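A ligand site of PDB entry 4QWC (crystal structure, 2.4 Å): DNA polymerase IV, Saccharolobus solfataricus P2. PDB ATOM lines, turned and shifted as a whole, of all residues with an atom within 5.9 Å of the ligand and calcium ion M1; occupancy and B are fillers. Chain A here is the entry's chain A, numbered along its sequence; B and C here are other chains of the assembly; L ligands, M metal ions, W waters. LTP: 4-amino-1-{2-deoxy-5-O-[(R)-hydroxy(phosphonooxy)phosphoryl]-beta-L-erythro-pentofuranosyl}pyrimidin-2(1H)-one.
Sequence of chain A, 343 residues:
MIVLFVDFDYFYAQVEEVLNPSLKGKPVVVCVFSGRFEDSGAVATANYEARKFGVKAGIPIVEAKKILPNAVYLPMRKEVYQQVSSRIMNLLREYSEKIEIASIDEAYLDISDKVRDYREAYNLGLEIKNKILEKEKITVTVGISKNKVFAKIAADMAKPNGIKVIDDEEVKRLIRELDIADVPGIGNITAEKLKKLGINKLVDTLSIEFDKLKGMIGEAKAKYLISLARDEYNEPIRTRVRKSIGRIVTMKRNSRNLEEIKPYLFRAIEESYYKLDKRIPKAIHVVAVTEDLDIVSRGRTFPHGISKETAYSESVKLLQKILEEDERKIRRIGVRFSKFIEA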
ATOM      1  N   ASP A   7     -17.492  -5.263 -28.173  1.00  0.00           N
ATOM      2  CA  ASP A   7     -17.075  -4.183 -27.319  1.00  0.00           C
ATOM      3  C   ASP A   7     -16.559  -4.711 -25.990  1.00  0.00           C
ATOM      4  O   ASP A   7     -17.341  -5.248 -25.214  1.00  0.00           O
ATOM      5  CB  ASP A   7     -18.266  -3.274 -27.065  1.00  0.00           C
ATOM      6  CG  ASP A   7     -17.872  -1.999 -26.344  1.00  0.00           C
ATOM      7  OD1 ASP A   7     -16.900  -2.018 -25.542  1.00  0.00           O
ATOM      8  OD2 ASP A   7     -18.549  -0.964 -26.580  1.00  0.00           O
ATOM      9  N   PHE A   8     -15.271  -4.532 -25.700  1.00  0.00           N
ATOM     10  CA  PHE A   8     -14.730  -5.104 -24.473  1.00  0.00           C
ATOM     11  C   PHE A   8     -15.318  -4.309 -23.312  1.00  0.00           C
ATOM     12  O   PHE A   8     -15.399  -3.076 -23.382  1.00  0.00           O
ATOM     13  CB  PHE A   8     -13.196  -5.055 -24.413  1.00  0.00           C
ATOM     14  CG  PHE A   8     -12.499  -5.478 -25.668  1.00  0.00           C
ATOM     15  CD1 PHE A   8     -13.108  -6.267 -26.626  1.00  0.00           C
ATOM     16  CD2 PHE A   8     -11.190  -5.083 -25.883  1.00  0.00           C
ATOM     17  CE1 PHE A   8     -12.439  -6.619 -27.774  1.00  0.00           C
ATOM     18  CE2 PHE A   8     -10.503  -5.456 -27.020  1.00  0.00           C
ATOM     19  CZ  PHE A   8     -11.111  -6.211 -27.967  1.00  0.00           C
ATOM     20  N   ASP A   9     -15.743  -5.004 -22.252  1.00  0.00           N
ATOM     21  CA  ASP A   9     -16.422  -4.370 -21.113  1.00  0.00           C
ATOM     22  C   ASP A   9     -15.410  -3.680 -20.200  1.00  0.00           C
ATOM     23  O   ASP A   9     -14.344  -4.231 -19.918  1.00  0.00           O
ATOM     24  CB  ASP A   9     -17.155  -5.411 -20.275  1.00  0.00           C
ATOM     25  CG  ASP A   9     -18.332  -6.068 -21.009  1.00  0.00           C
ATOM     26  OD1 ASP A   9     -18.965  -5.452 -21.904  1.00  0.00           O
ATOM     27  OD2 ASP A   9     -18.667  -7.199 -20.639  1.00  0.00           O
ATOM     28  N   TYR A  10     -15.769  -2.467 -19.751  1.00  0.00           N
ATOM     29  CA  TYR A  10     -14.961  -1.656 -18.810  1.00  0.00           C
ATOM     30  C   TYR A  10     -13.432  -1.923 -18.893  1.00  0.00           C
ATOM     31  O   TYR A  10     -12.737  -2.176 -17.915  1.00  0.00           O
ATOM     32  CB  TYR A  10     -15.538  -1.743 -17.372  1.00  0.00           C
ATOM     33  CG  TYR A  10     -15.563  -3.138 -16.765  1.00  0.00           C
ATOM     34  CD1 TYR A  10     -16.581  -4.038 -17.074  1.00  0.00           C
ATOM     35  CD2 TYR A  10     -14.586  -3.532 -15.847  1.00  0.00           C
ATOM     36  CE1 TYR A  10     -16.599  -5.314 -16.522  1.00  0.00           C
ATOM     37  CE2 TYR A  10     -14.602  -4.796 -15.275  1.00  0.00           C
ATOM     38  CZ  TYR A  10     -15.610  -5.681 -15.626  1.00  0.00           C
ATOM     39  OH  TYR A  10     -15.608  -6.934 -15.063  1.00  0.00           O
ATOM     40  N   PHE A  11     -12.932  -1.782 -20.120  1.00  0.00           N
ATOM     41  CA  PHE A  11     -11.711  -2.445 -20.553  1.00  0.00           C
ATOM     42  C   PHE A  11     -10.454  -2.127 -19.733  1.00  0.00           C
ATOM     43  O   PHE A  11      -9.798  -3.046 -19.229  1.00  0.00           O
ATOM     44  CB  PHE A  11     -11.491  -2.161 -22.054  1.00  0.00           C
ATOM     45  CG  PHE A  11     -10.285  -2.836 -22.629  1.00  0.00           C
ATOM     46  CD1 PHE A  11     -10.114  -4.197 -22.515  1.00  0.00           C
ATOM     47  CD2 PHE A  11      -9.306  -2.109 -23.276  1.00  0.00           C
ATOM     48  CE1 PHE A  11      -8.982  -4.831 -23.049  1.00  0.00           C
ATOM     49  CE2 PHE A  11      -8.196  -2.729 -23.827  1.00  0.00           C
ATOM     50  CZ  PHE A  11      -8.032  -4.091 -23.705  1.00  0.00           C
ATOM     51  N   TYR A  12     -10.095  -0.870 -19.581  1.00  0.00           N
ATOM     52  CA  TYR A  12      -8.910  -0.556 -18.788  1.00  0.00           C
ATOM     53  C   TYR A  12      -8.998  -1.115 -17.358  1.00  0.00           C
ATOM     54  O   TYR A  12      -8.029  -1.660 -16.814  1.00  0.00           O
ATOM     55  CB  TYR A  12      -8.642   0.941 -18.705  1.00  0.00           C
ATOM     56  CG  TYR A  12      -8.467   1.668 -20.003  1.00  0.00           C
ATOM     57  CD1 TYR A  12      -8.226   0.981 -21.202  1.00  0.00           C
ATOM     58  CD2 TYR A  12      -8.494   3.053 -20.033  1.00  0.00           C
ATOM     59  CE1 TYR A  12      -8.042   1.679 -22.375  1.00  0.00           C
ATOM     60  CE2 TYR A  12      -8.298   3.747 -21.210  1.00  0.00           C
ATOM     61  CZ  TYR A  12      -8.067   3.043 -22.367  1.00  0.00           C
ATOM     62  OH  TYR A  12      -7.911   3.731 -23.541  1.00  0.00           O
ATOM     63  N   VAL A  43     -11.195  10.656 -14.475  1.00  0.00           N
ATOM     64  CA  VAL A  43     -11.422   9.222 -14.557  1.00  0.00           C
ATOM     65  C   VAL A  43     -11.546   8.853 -16.015  1.00  0.00           C
ATOM     66  O   VAL A  43     -12.384   9.405 -16.743  1.00  0.00           O
ATOM     67  CB  VAL A  43     -12.740   8.819 -13.863  1.00  0.00           C
ATOM     68  CG1 VAL A  43     -13.038   7.352 -14.091  1.00  0.00           C
ATOM     69  CG2 VAL A  43     -12.670   9.146 -12.370  1.00  0.00           C
ATOM     70  N   ALA A  44     -10.718   7.908 -16.451  1.00  0.00           N
ATOM     71  CA  ALA A  44     -10.749   7.444 -17.836  1.00  0.00           C
ATOM     72  C   ALA A  44     -11.791   6.354 -17.917  1.00  0.00           C
ATOM     73  O   ALA A  44     -12.619   6.327 -18.837  1.00  0.00           O
ATOM     74  CB  ALA A  44      -9.381   6.912 -18.204  1.00  0.00           C
ATOM     75  N   THR A  45     -11.803   5.477 -16.917  1.00  0.00           N
ATOM     76  CA  THR A  45     -12.873   4.502 -16.808  1.00  0.00           C
ATOM     77  C   THR A  45     -12.968   3.891 -15.414  1.00  0.00           C
ATOM     78  O   THR A  45     -12.018   3.870 -14.660  1.00  0.00           O
ATOM     79  CB  THR A  45     -12.687   3.353 -17.818  1.00  0.00           C
ATOM     80  OG1 THR A  45     -13.684   2.334 -17.612  1.00  0.00           O
ATOM     81  CG2 THR A  45     -11.344   2.721 -17.610  1.00  0.00           C
ATOM     82  N   ALA A  46     -14.127   3.355 -15.116  1.00  0.00           N
ATOM     83  CA  ALA A  46     -14.345   2.652 -13.864  1.00  0.00           C
ATOM     84  C   ALA A  46     -15.017   1.295 -14.128  1.00  0.00           C
ATOM     85  O   ALA A  46     -15.728   1.136 -15.118  1.00  0.00           O
ATOM     86  CB  ALA A  46     -15.214   3.505 -12.949  1.00  0.00           C
ATOM     87  N   TYR A  48     -17.873  -1.737 -13.124  1.00  0.00           N
ATOM     88  CA  TYR A  48     -19.322  -1.555 -12.838  1.00  0.00           C
ATOM     89  C   TYR A  48     -19.643  -1.400 -11.355  1.00  0.00           C
ATOM     90  O   TYR A  48     -20.629  -0.743 -11.000  1.00  0.00           O
ATOM     91  CB  TYR A  48     -20.165  -2.628 -13.512  1.00  0.00           C
ATOM     92  CG  TYR A  48     -20.425  -2.297 -14.970  1.00  0.00           C
ATOM     93  CD1 TYR A  48     -19.474  -2.558 -15.940  1.00  0.00           C
ATOM     94  CD2 TYR A  48     -21.602  -1.655 -15.358  1.00  0.00           C
ATOM     95  CE1 TYR A  48     -19.688  -2.223 -17.271  1.00  0.00           C
ATOM     96  CE2 TYR A  48     -21.829  -1.315 -16.685  1.00  0.00           C
ATOM     97  CZ  TYR A  48     -20.860  -1.597 -17.644  1.00  0.00           C
ATOM     98  OH  TYR A  48     -21.074  -1.261 -18.974  1.00  0.00           O
ATOM     99  N   ARG A  51     -19.242   2.247 -11.007  1.00  0.00           N
ATOM    100  CA  ARG A  51     -20.262   2.963 -11.771  1.00  0.00           C
ATOM    101  C   ARG A  51     -21.607   2.990 -11.071  1.00  0.00           C
ATOM    102  O   ARG A  51     -22.395   3.892 -11.297  1.00  0.00           O
ATOM    103  CB  ARG A  51     -20.440   2.342 -13.158  1.00  0.00           C
ATOM    104  CG  ARG A  51     -19.233   2.507 -14.055  1.00  0.00           C
ATOM    105  CD  ARG A  51     -19.573   2.182 -15.506  1.00  0.00           C
ATOM    106  NE  ARG A  51     -18.369   2.024 -16.307  1.00  0.00           N
ATOM    107  CZ  ARG A  51     -18.353   1.608 -17.563  1.00  0.00           C
ATOM    108  NH1 ARG A  51     -19.472   1.289 -18.199  1.00  0.00           N
ATOM    109  NH2 ARG A  51     -17.195   1.495 -18.198  1.00  0.00           N
ATOM    110  N   ALA A  57     -16.524   7.704 -16.368  1.00  0.00           N
ATOM    111  CA  ALA A  57     -15.556   8.358 -17.256  1.00  0.00           C
ATOM    112  C   ALA A  57     -15.836   9.846 -17.435  1.00  0.00           C
ATOM    113  O   ALA A  57     -16.957  10.246 -17.758  1.00  0.00           O
ATOM    114  CB  ALA A  57     -15.554   7.654 -18.613  1.00  0.00           C
ATOM    115  N   GLY A  58     -14.808  10.665 -17.224  1.00  0.00           N
ATOM    116  CA  GLY A  58     -14.900  12.122 -17.419  1.00  0.00           C
ATOM    117  C   GLY A  58     -14.974  12.939 -16.137  1.00  0.00           C
ATOM    118  O   GLY A  58     -14.572  14.090 -16.130  1.00  0.00           O
ATOM    119  N   MET A  76      -3.724   5.276 -15.255  1.00  0.00           N
ATOM    120  CA  MET A  76      -3.718   4.727 -16.589  1.00  0.00           C
ATOM    121  C   MET A  76      -2.383   4.169 -17.038  1.00  0.00           C
ATOM    122  O   MET A  76      -1.359   4.830 -16.964  1.00  0.00           O
ATOM    123  CB  MET A  76      -4.081   5.806 -17.613  1.00  0.00           C
ATOM    124  CG  MET A  76      -5.489   5.642 -18.148  1.00  0.00           C
ATOM    125  SD  MET A  76      -5.558   5.866 -19.923  1.00  0.00           S
ATOM    126  CE  MET A  76      -4.507   7.319 -20.201  1.00  0.00           C
ATOM    127  N   SER A 103     -11.561   1.170 -32.275  1.00  0.00           N
ATOM    128  CA  SER A 103     -10.864   1.790 -31.159  1.00  0.00           C
ATOM    129  C   SER A 103     -10.117   0.714 -30.478  1.00  0.00           C
ATOM    130  O   SER A 103     -10.135  -0.449 -30.913  1.00  0.00           O
ATOM    131  CB  SER A 103     -11.838   2.412 -30.159  1.00  0.00           C
ATOM    132  OG  SER A 103     -12.575   1.415 -29.451  1.00  0.00           O
ATOM    133  N   ILE A 104      -9.487   1.079 -29.361  1.00  0.00           N
ATOM    134  CA  ILE A 104      -8.710   0.124 -28.573  1.00  0.00           C
ATOM    135  C   ILE A 104      -9.569  -1.013 -28.021  1.00  0.00           C
ATOM    136  O   ILE A 104      -9.033  -2.069 -27.643  1.00  0.00           O
ATOM    137  CB  ILE A 104      -8.004   0.850 -27.431  1.00  0.00           C
ATOM    138  CG1 ILE A 104      -6.939  -0.028 -26.785  1.00  0.00           C
ATOM    139  CG2 ILE A 104      -8.999   1.322 -26.384  1.00  0.00           C
ATOM    140  CD1 ILE A 104      -6.034   0.743 -25.836  1.00  0.00           C
ATOM    141  N   ASP A 105     -10.888  -0.851 -27.971  1.00  0.00           N
ATOM    142  CA  ASP A 105     -11.706  -1.916 -27.429  1.00  0.00           C
ATOM    143  C   ASP A 105     -13.016  -2.184 -28.199  1.00  0.00           C
ATOM    144  O   ASP A 105     -14.016  -2.622 -27.611  1.00  0.00           O
ATOM    145  CB  ASP A 105     -11.997  -1.630 -25.963  1.00  0.00           C
ATOM    146  CG  ASP A 105     -13.127  -0.693 -25.784  1.00  0.00           C
ATOM    147  OD1 ASP A 105     -13.234   0.214 -26.633  1.00  0.00           O
ATOM    148  OD2 ASP A 105     -13.959  -0.876 -24.836  1.00  0.00           O
ATOM    149  N   GLU A 106     -12.992  -1.925 -29.499  1.00  0.00           N
ATOM    150  CA  GLU A 106     -14.181  -2.094 -30.335  1.00  0.00           C
ATOM    151  C   GLU A 106     -13.771  -2.560 -31.717  1.00  0.00           C
ATOM    152  O   GLU A 106     -12.830  -2.025 -32.289  1.00  0.00           O
ATOM    153  CB  GLU A 106     -14.898  -0.767 -30.536  1.00  0.00           C
ATOM    154  CG  GLU A 106     -15.534  -0.132 -29.329  1.00  0.00           C
ATOM    155  CD  GLU A 106     -16.018   1.272 -29.666  1.00  0.00           C
ATOM    156  OE1 GLU A 106     -15.174   2.208 -29.719  1.00  0.00           O
ATOM    157  OE2 GLU A 106     -17.222   1.432 -29.929  1.00  0.00           O
ATOM    158  N   LYS A 159     -24.677  -4.435 -22.865  1.00  0.00           N
ATOM    159  CA  LYS A 159     -23.510  -4.415 -21.981  1.00  0.00           C
ATOM    160  C   LYS A 159     -23.910  -4.209 -20.515  1.00  0.00           C
ATOM    161  O   LYS A 159     -24.915  -3.540 -20.243  1.00  0.00           O
ATOM    162  CB  LYS A 159     -22.459  -3.377 -22.412  1.00  0.00           C
ATOM    163  CG  LYS A 159     -22.912  -1.919 -22.466  1.00  0.00           C
ATOM    164  CD  LYS A 159     -21.723  -0.980 -22.686  1.00  0.00           C
ATOM    165  CE  LYS A 159     -21.004  -1.236 -24.010  1.00  0.00           C
ATOM    166  NZ  LYS A 159     -19.849  -0.285 -24.201  1.00  0.00           N
ATOM    167  P    DG B   5      -7.527  18.734 -15.770  1.00  0.00           P
ATOM    168  OP1  DG B   5      -6.777  19.377 -14.668  1.00  0.00           O
ATOM    169  OP2  DG B   5      -7.667  19.409 -17.084  1.00  0.00           O
ATOM    170  O5'  DG B   5      -6.848  17.323 -15.980  1.00  0.00           O
ATOM    171  C5'  DG B   5      -7.493  16.328 -16.782  1.00  0.00           C
ATOM    172  C4'  DG B   5      -6.479  15.318 -17.246  1.00  0.00           C
ATOM    173  O4'  DG B   5      -7.171  14.130 -17.701  1.00  0.00           O
ATOM    174  C3'  DG B   5      -5.650  15.755 -18.441  1.00  0.00           C
ATOM    175  O3'  DG B   5      -4.465  14.943 -18.434  1.00  0.00           O
ATOM    176  C2'  DG B   5      -6.586  15.460 -19.598  1.00  0.00           C
ATOM    177  C1'  DG B   5      -7.297  14.188 -19.117  1.00  0.00           C
ATOM    178  N9   DG B   5      -8.722  14.071 -19.445  1.00  0.00           N
ATOM    179  C8   DG B   5      -9.691  15.036 -19.345  1.00  0.00           C
ATOM    180  N7   DG B   5     -10.871  14.604 -19.679  1.00  0.00           N
ATOM    181  C5   DG B   5     -10.671  13.267 -19.992  1.00  0.00           C
ATOM    182  C6   DG B   5     -11.590  12.272 -20.433  1.00  0.00           C
ATOM    183  O6   DG B   5     -12.811  12.382 -20.628  1.00  0.00           O
ATOM    184  N1   DG B   5     -10.960  11.059 -20.644  1.00  0.00           N
ATOM    185  C2   DG B   5      -9.618  10.817 -20.472  1.00  0.00           C
ATOM    186  N2   DG B   5      -9.194   9.571 -20.732  1.00  0.00           N
ATOM    187  N3   DG B   5      -8.758  11.726 -20.042  1.00  0.00           N
ATOM    188  C4   DG B   5      -9.350  12.925 -19.842  1.00  0.00           C
ATOM    189  P    DG B   6      -3.252  15.210 -19.448  1.00  0.00           P
ATOM    190  OP1  DG B   6      -2.020  14.667 -18.813  1.00  0.00           O
ATOM    191  OP2  DG B   6      -3.313  16.617 -19.909  1.00  0.00           O
ATOM    192  O5'  DG B   6      -3.607  14.295 -20.698  1.00  0.00           O
ATOM    193  C5'  DG B   6      -3.407  12.873 -20.617  1.00  0.00           C
ATOM    194  C4'  DG B   6      -4.067  12.187 -21.787  1.00  0.00           C
ATOM    195  O4'  DG B   6      -5.491  12.417 -21.786  1.00  0.00           O
ATOM    196  C3'  DG B   6      -3.560  12.687 -23.152  1.00  0.00           C
ATOM    197  O3'  DG B   6      -2.889  11.606 -23.789  1.00  0.00           O
ATOM    198  C2'  DG B   6      -4.817  13.148 -23.878  1.00  0.00           C
ATOM    199  C1'  DG B   6      -5.910  12.417 -23.128  1.00  0.00           C
ATOM    200  N9   DG B   6      -7.235  13.034 -23.199  1.00  0.00           N
ATOM    201  C8   DG B   6      -7.568  14.346 -22.962  1.00  0.00           C
ATOM    202  N7   DG B   6      -8.836  14.597 -23.131  1.00  0.00           N
ATOM    203  C5   DG B   6      -9.365  13.374 -23.515  1.00  0.00           C
ATOM    204  C6   DG B   6     -10.701  13.023 -23.843  1.00  0.00           C
ATOM    205  O6   DG B   6     -11.711  13.742 -23.855  1.00  0.00           O
ATOM    206  N1   DG B   6     -10.812  11.672 -24.184  1.00  0.00           N
ATOM    207  C2   DG B   6      -9.761  10.784 -24.213  1.00  0.00           C
ATOM    208  N2   DG B   6     -10.048   9.524 -24.579  1.00  0.00           N
ATOM    209  N3   DG B   6      -8.517  11.100 -23.911  1.00  0.00           N
ATOM    210  C4   DG B   6      -8.395  12.402 -23.574  1.00  0.00           C
ATOM    211  N1  DOC C  13     -14.685   9.394 -25.679  1.00  0.00           N
ATOM    212  C2  DOC C  13     -13.407   9.845 -25.304  1.00  0.00           C
ATOM    213  N3  DOC C  13     -13.264  11.053 -24.711  1.00  0.00           N
ATOM    214  C4  DOC C  13     -14.345  11.835 -24.476  1.00  0.00           C
ATOM    215  C5  DOC C  13     -15.609  11.413 -24.844  1.00  0.00           C
ATOM    216  C6  DOC C  13     -15.759  10.178 -25.452  1.00  0.00           C
ATOM    217  O2  DOC C  13     -12.390   9.146 -25.518  1.00  0.00           O
ATOM    218  N4  DOC C  13     -14.177  13.033 -23.890  1.00  0.00           N
ATOM    219  C1' DOC C  13     -14.812   8.078 -26.346  1.00  0.00           C
ATOM    220  C2' DOC C  13     -14.275   6.906 -25.525  1.00  0.00           C
ATOM    221  C3' DOC C  13     -15.380   5.874 -25.494  1.00  0.00           C
ATOM    222  C4' DOC C  13     -16.472   6.412 -26.406  1.00  0.00           C
ATOM    223  O4' DOC C  13     -16.181   7.789 -26.604  1.00  0.00           O
ATOM    224  C5' DOC C  13     -17.872   6.313 -25.809  1.00  0.00           C
ATOM    225  O5' DOC C  13     -18.848   6.676 -26.792  1.00  0.00           O
ATOM    226  P   DOC C  13     -19.256   5.687 -27.987  1.00  0.00           P
ATOM    227  OP1 DOC C  13     -18.328   4.481 -27.988  1.00  0.00           O
ATOM    228  OP2 DOC C  13     -20.741   5.431 -27.867  1.00  0.00           O
HETATM  229  OAE LTP L   1     -17.479   0.509 -23.182  1.00  0.00           O
HETATM  230  PAF LTP L   1     -17.680   1.677 -22.248  1.00  0.00           P
HETATM  231  OAG LTP L   1     -19.039   1.748 -21.605  1.00  0.00           O
HETATM  232  OBB LTP L   1     -17.122   2.974 -22.781  1.00  0.00           O
HETATM  233  OAH LTP L   1     -16.753   1.353 -20.992  1.00  0.00           O
HETATM  234  PAI LTP L   1     -15.192   1.238 -21.250  1.00  0.00           P
HETATM  235  OAJ LTP L   1     -14.921  -0.104 -21.891  1.00  0.00           O
HETATM  236  OAK LTP L   1     -14.579   1.584 -19.918  1.00  0.00           O
HETATM  237  OAL LTP L   1     -14.798   2.438 -22.287  1.00  0.00           O
HETATM  238  CAM LTP L   1     -13.843   2.293 -23.372  1.00  0.00           C
HETATM  239  CAN LTP L   1     -12.478   2.899 -23.065  1.00  0.00           C
HETATM  240  OAO LTP L   1     -12.580   3.796 -21.967  1.00  0.00           O
HETATM  241  CAP LTP L   1     -11.861   3.694 -24.225  1.00  0.00           C
HETATM  242  O12 LTP L   1     -10.783   2.991 -24.859  1.00  0.00           O
HETATM  243  CAQ LTP L   1     -11.300   4.949 -23.634  1.00  0.00           C
HETATM  244  CAR LTP L   1     -11.754   4.947 -22.181  1.00  0.00           C
HETATM  245  N1  LTP L   1     -12.472   6.205 -22.039  1.00  0.00           N
HETATM  246  C2  LTP L   1     -11.758   7.337 -21.902  1.00  0.00           C
HETATM  247  O2  LTP L   1     -10.494   7.346 -21.854  1.00  0.00           O
HETATM  248  C6  LTP L   1     -13.954   6.205 -22.091  1.00  0.00           C
HETATM  249  C5  LTP L   1     -14.528   7.540 -21.988  1.00  0.00           C
HETATM  250  C4  LTP L   1     -13.708   8.654 -21.841  1.00  0.00           C
HETATM  251  NAX LTP L   1     -14.223   9.906 -21.722  1.00  0.00           N
HETATM  252  N3  LTP L   1     -12.384   8.508 -21.812  1.00  0.00           N
HETATM  253 CA    CA M   1     -15.959  -0.938 -23.752  1.00  0.00          CA
HETATM  254 CA    CA M   2     -16.063   0.917 -25.924  1.00  0.00          CA
HETATM  255  O   HOH W   1     -11.914   1.171 -20.552  1.00  0.00           O
HETATM  256  O   HOH W   2     -18.407  -1.092 -20.621  1.00  0.00           O
HETATM  257  O   HOH W   3     -18.397  -3.223 -23.464  1.00  0.00           O
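An oxygen (OAK) of the ligand sits at hydrogen-bond distance from the side-chain hydroxyl of Thr 45. The side-chain amino group of Lys 159 is in salt-bridge range of an oxygen (OAG) of the ligand (3.4 Å). O6 of DG 5 of chain B lies within hydrogen-bond range of a nitrogen (NAX) of the ligand (3.1 Å). The guanidinium group of Arg 51 is in salt-bridge range of an oxygen (OAK) of the ligand (3.1 Å). The backbone NH (N) of Phe 11 sits close to an oxygen (OAJ) of the ligand. OH of Tyr 12 sits at hydrogen-bond distance from O12 of the ligand (3.2 Å). The backbone NH (N) of Tyr 10 lies close to an oxygen (OAJ) of the ligand, at 3.3 Å. N3 of DOC 13 of chain C is in hydrogen-bond range of NAX of the ligand (3.3 Å).
The side-chain carboxylate (OD1) of Asp 105 sits at hydrogen-bond distance from the side-chain hydroxyl (OG) of Ser 103 (3.1 Å). The side-chain carboxylate of Asp 7 is in salt-bridge range of the side-chain amino group of Lys 159 (2.8 Å). The guanidinium group of Arg 51 lies within hydrogen-bond range of the side-chain hydroxyl of Tyr 48, 3.1 Å away. The backbone carbonyl oxygen (O) of Ala 46 lies within hydrogen-bond range of the guanidinium group (NE) of Arg 51, at 3.0 Å. O2 of DOC 13 of chain C lies close to N2 of DG 6 of chain B (2.6 Å).
N1 of the ligand lies close to O of Ala 44, 3.2 Å away. Residues that only touch the ligand: Ile 104 (2.9 Å), DG 6 of chain B (3.5 Å), Ala 57 (3.5 Å) and Asp 9 (3.99 Å). Hydrophobic or aromatic side chains within 4 Å of the ligand: Tyr 12, Ala 44, Ala 57 and Ile 104. Of the 23 residues printed, 16 come within 4 Å of the ligand. The nearest printed residue that does not touch the ligand is Tyr 48 (4.5 Å).
Lys 159 touches calcium ion M1 (NZ to CA, 3.97 Å). Within 4 Å of calcium ion M1: Asp 7, Phe 8, Asp 105 and Lys 159. Along chain A the residues within 4 Å of calcium ion M1 span positions 7 to 159. The nearest printed residue that does not touch calcium ion M1 is Tyr 10 (4.3 Å).
Calcium ion M1 is bound by OAE of the ligand (2.2 Å), O of Phe 8 (2.2 Å), OD2 of Asp 105 (2.3 Å), OAJ of the ligand (2.3 Å) and OD1 of Asp 7 (2.3 Å).
Water W1 lies within hydrogen-bond range of an oxygen (OAK) of the ligand (2.8 Å), the backbone NH of Tyr 12 (2.9 Å) and the backbone NH of Phe 11 (3.2 Å). Water W2 lies within hydrogen-bond range of an oxygen (OAH) of the ligand, the backbone NH of Tyr 10 and the side-chain hydroxyl of Tyr 48. Water W3 lies within hydrogen-bond range of the side-chain carboxylate (OD1) of Asp 9 (2.8 Å), the backbone carbonyl oxygen (O) of Asp 7 (2.9 Å) and the side-chain amino group (NZ) of Lys 159 (3.4 Å).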
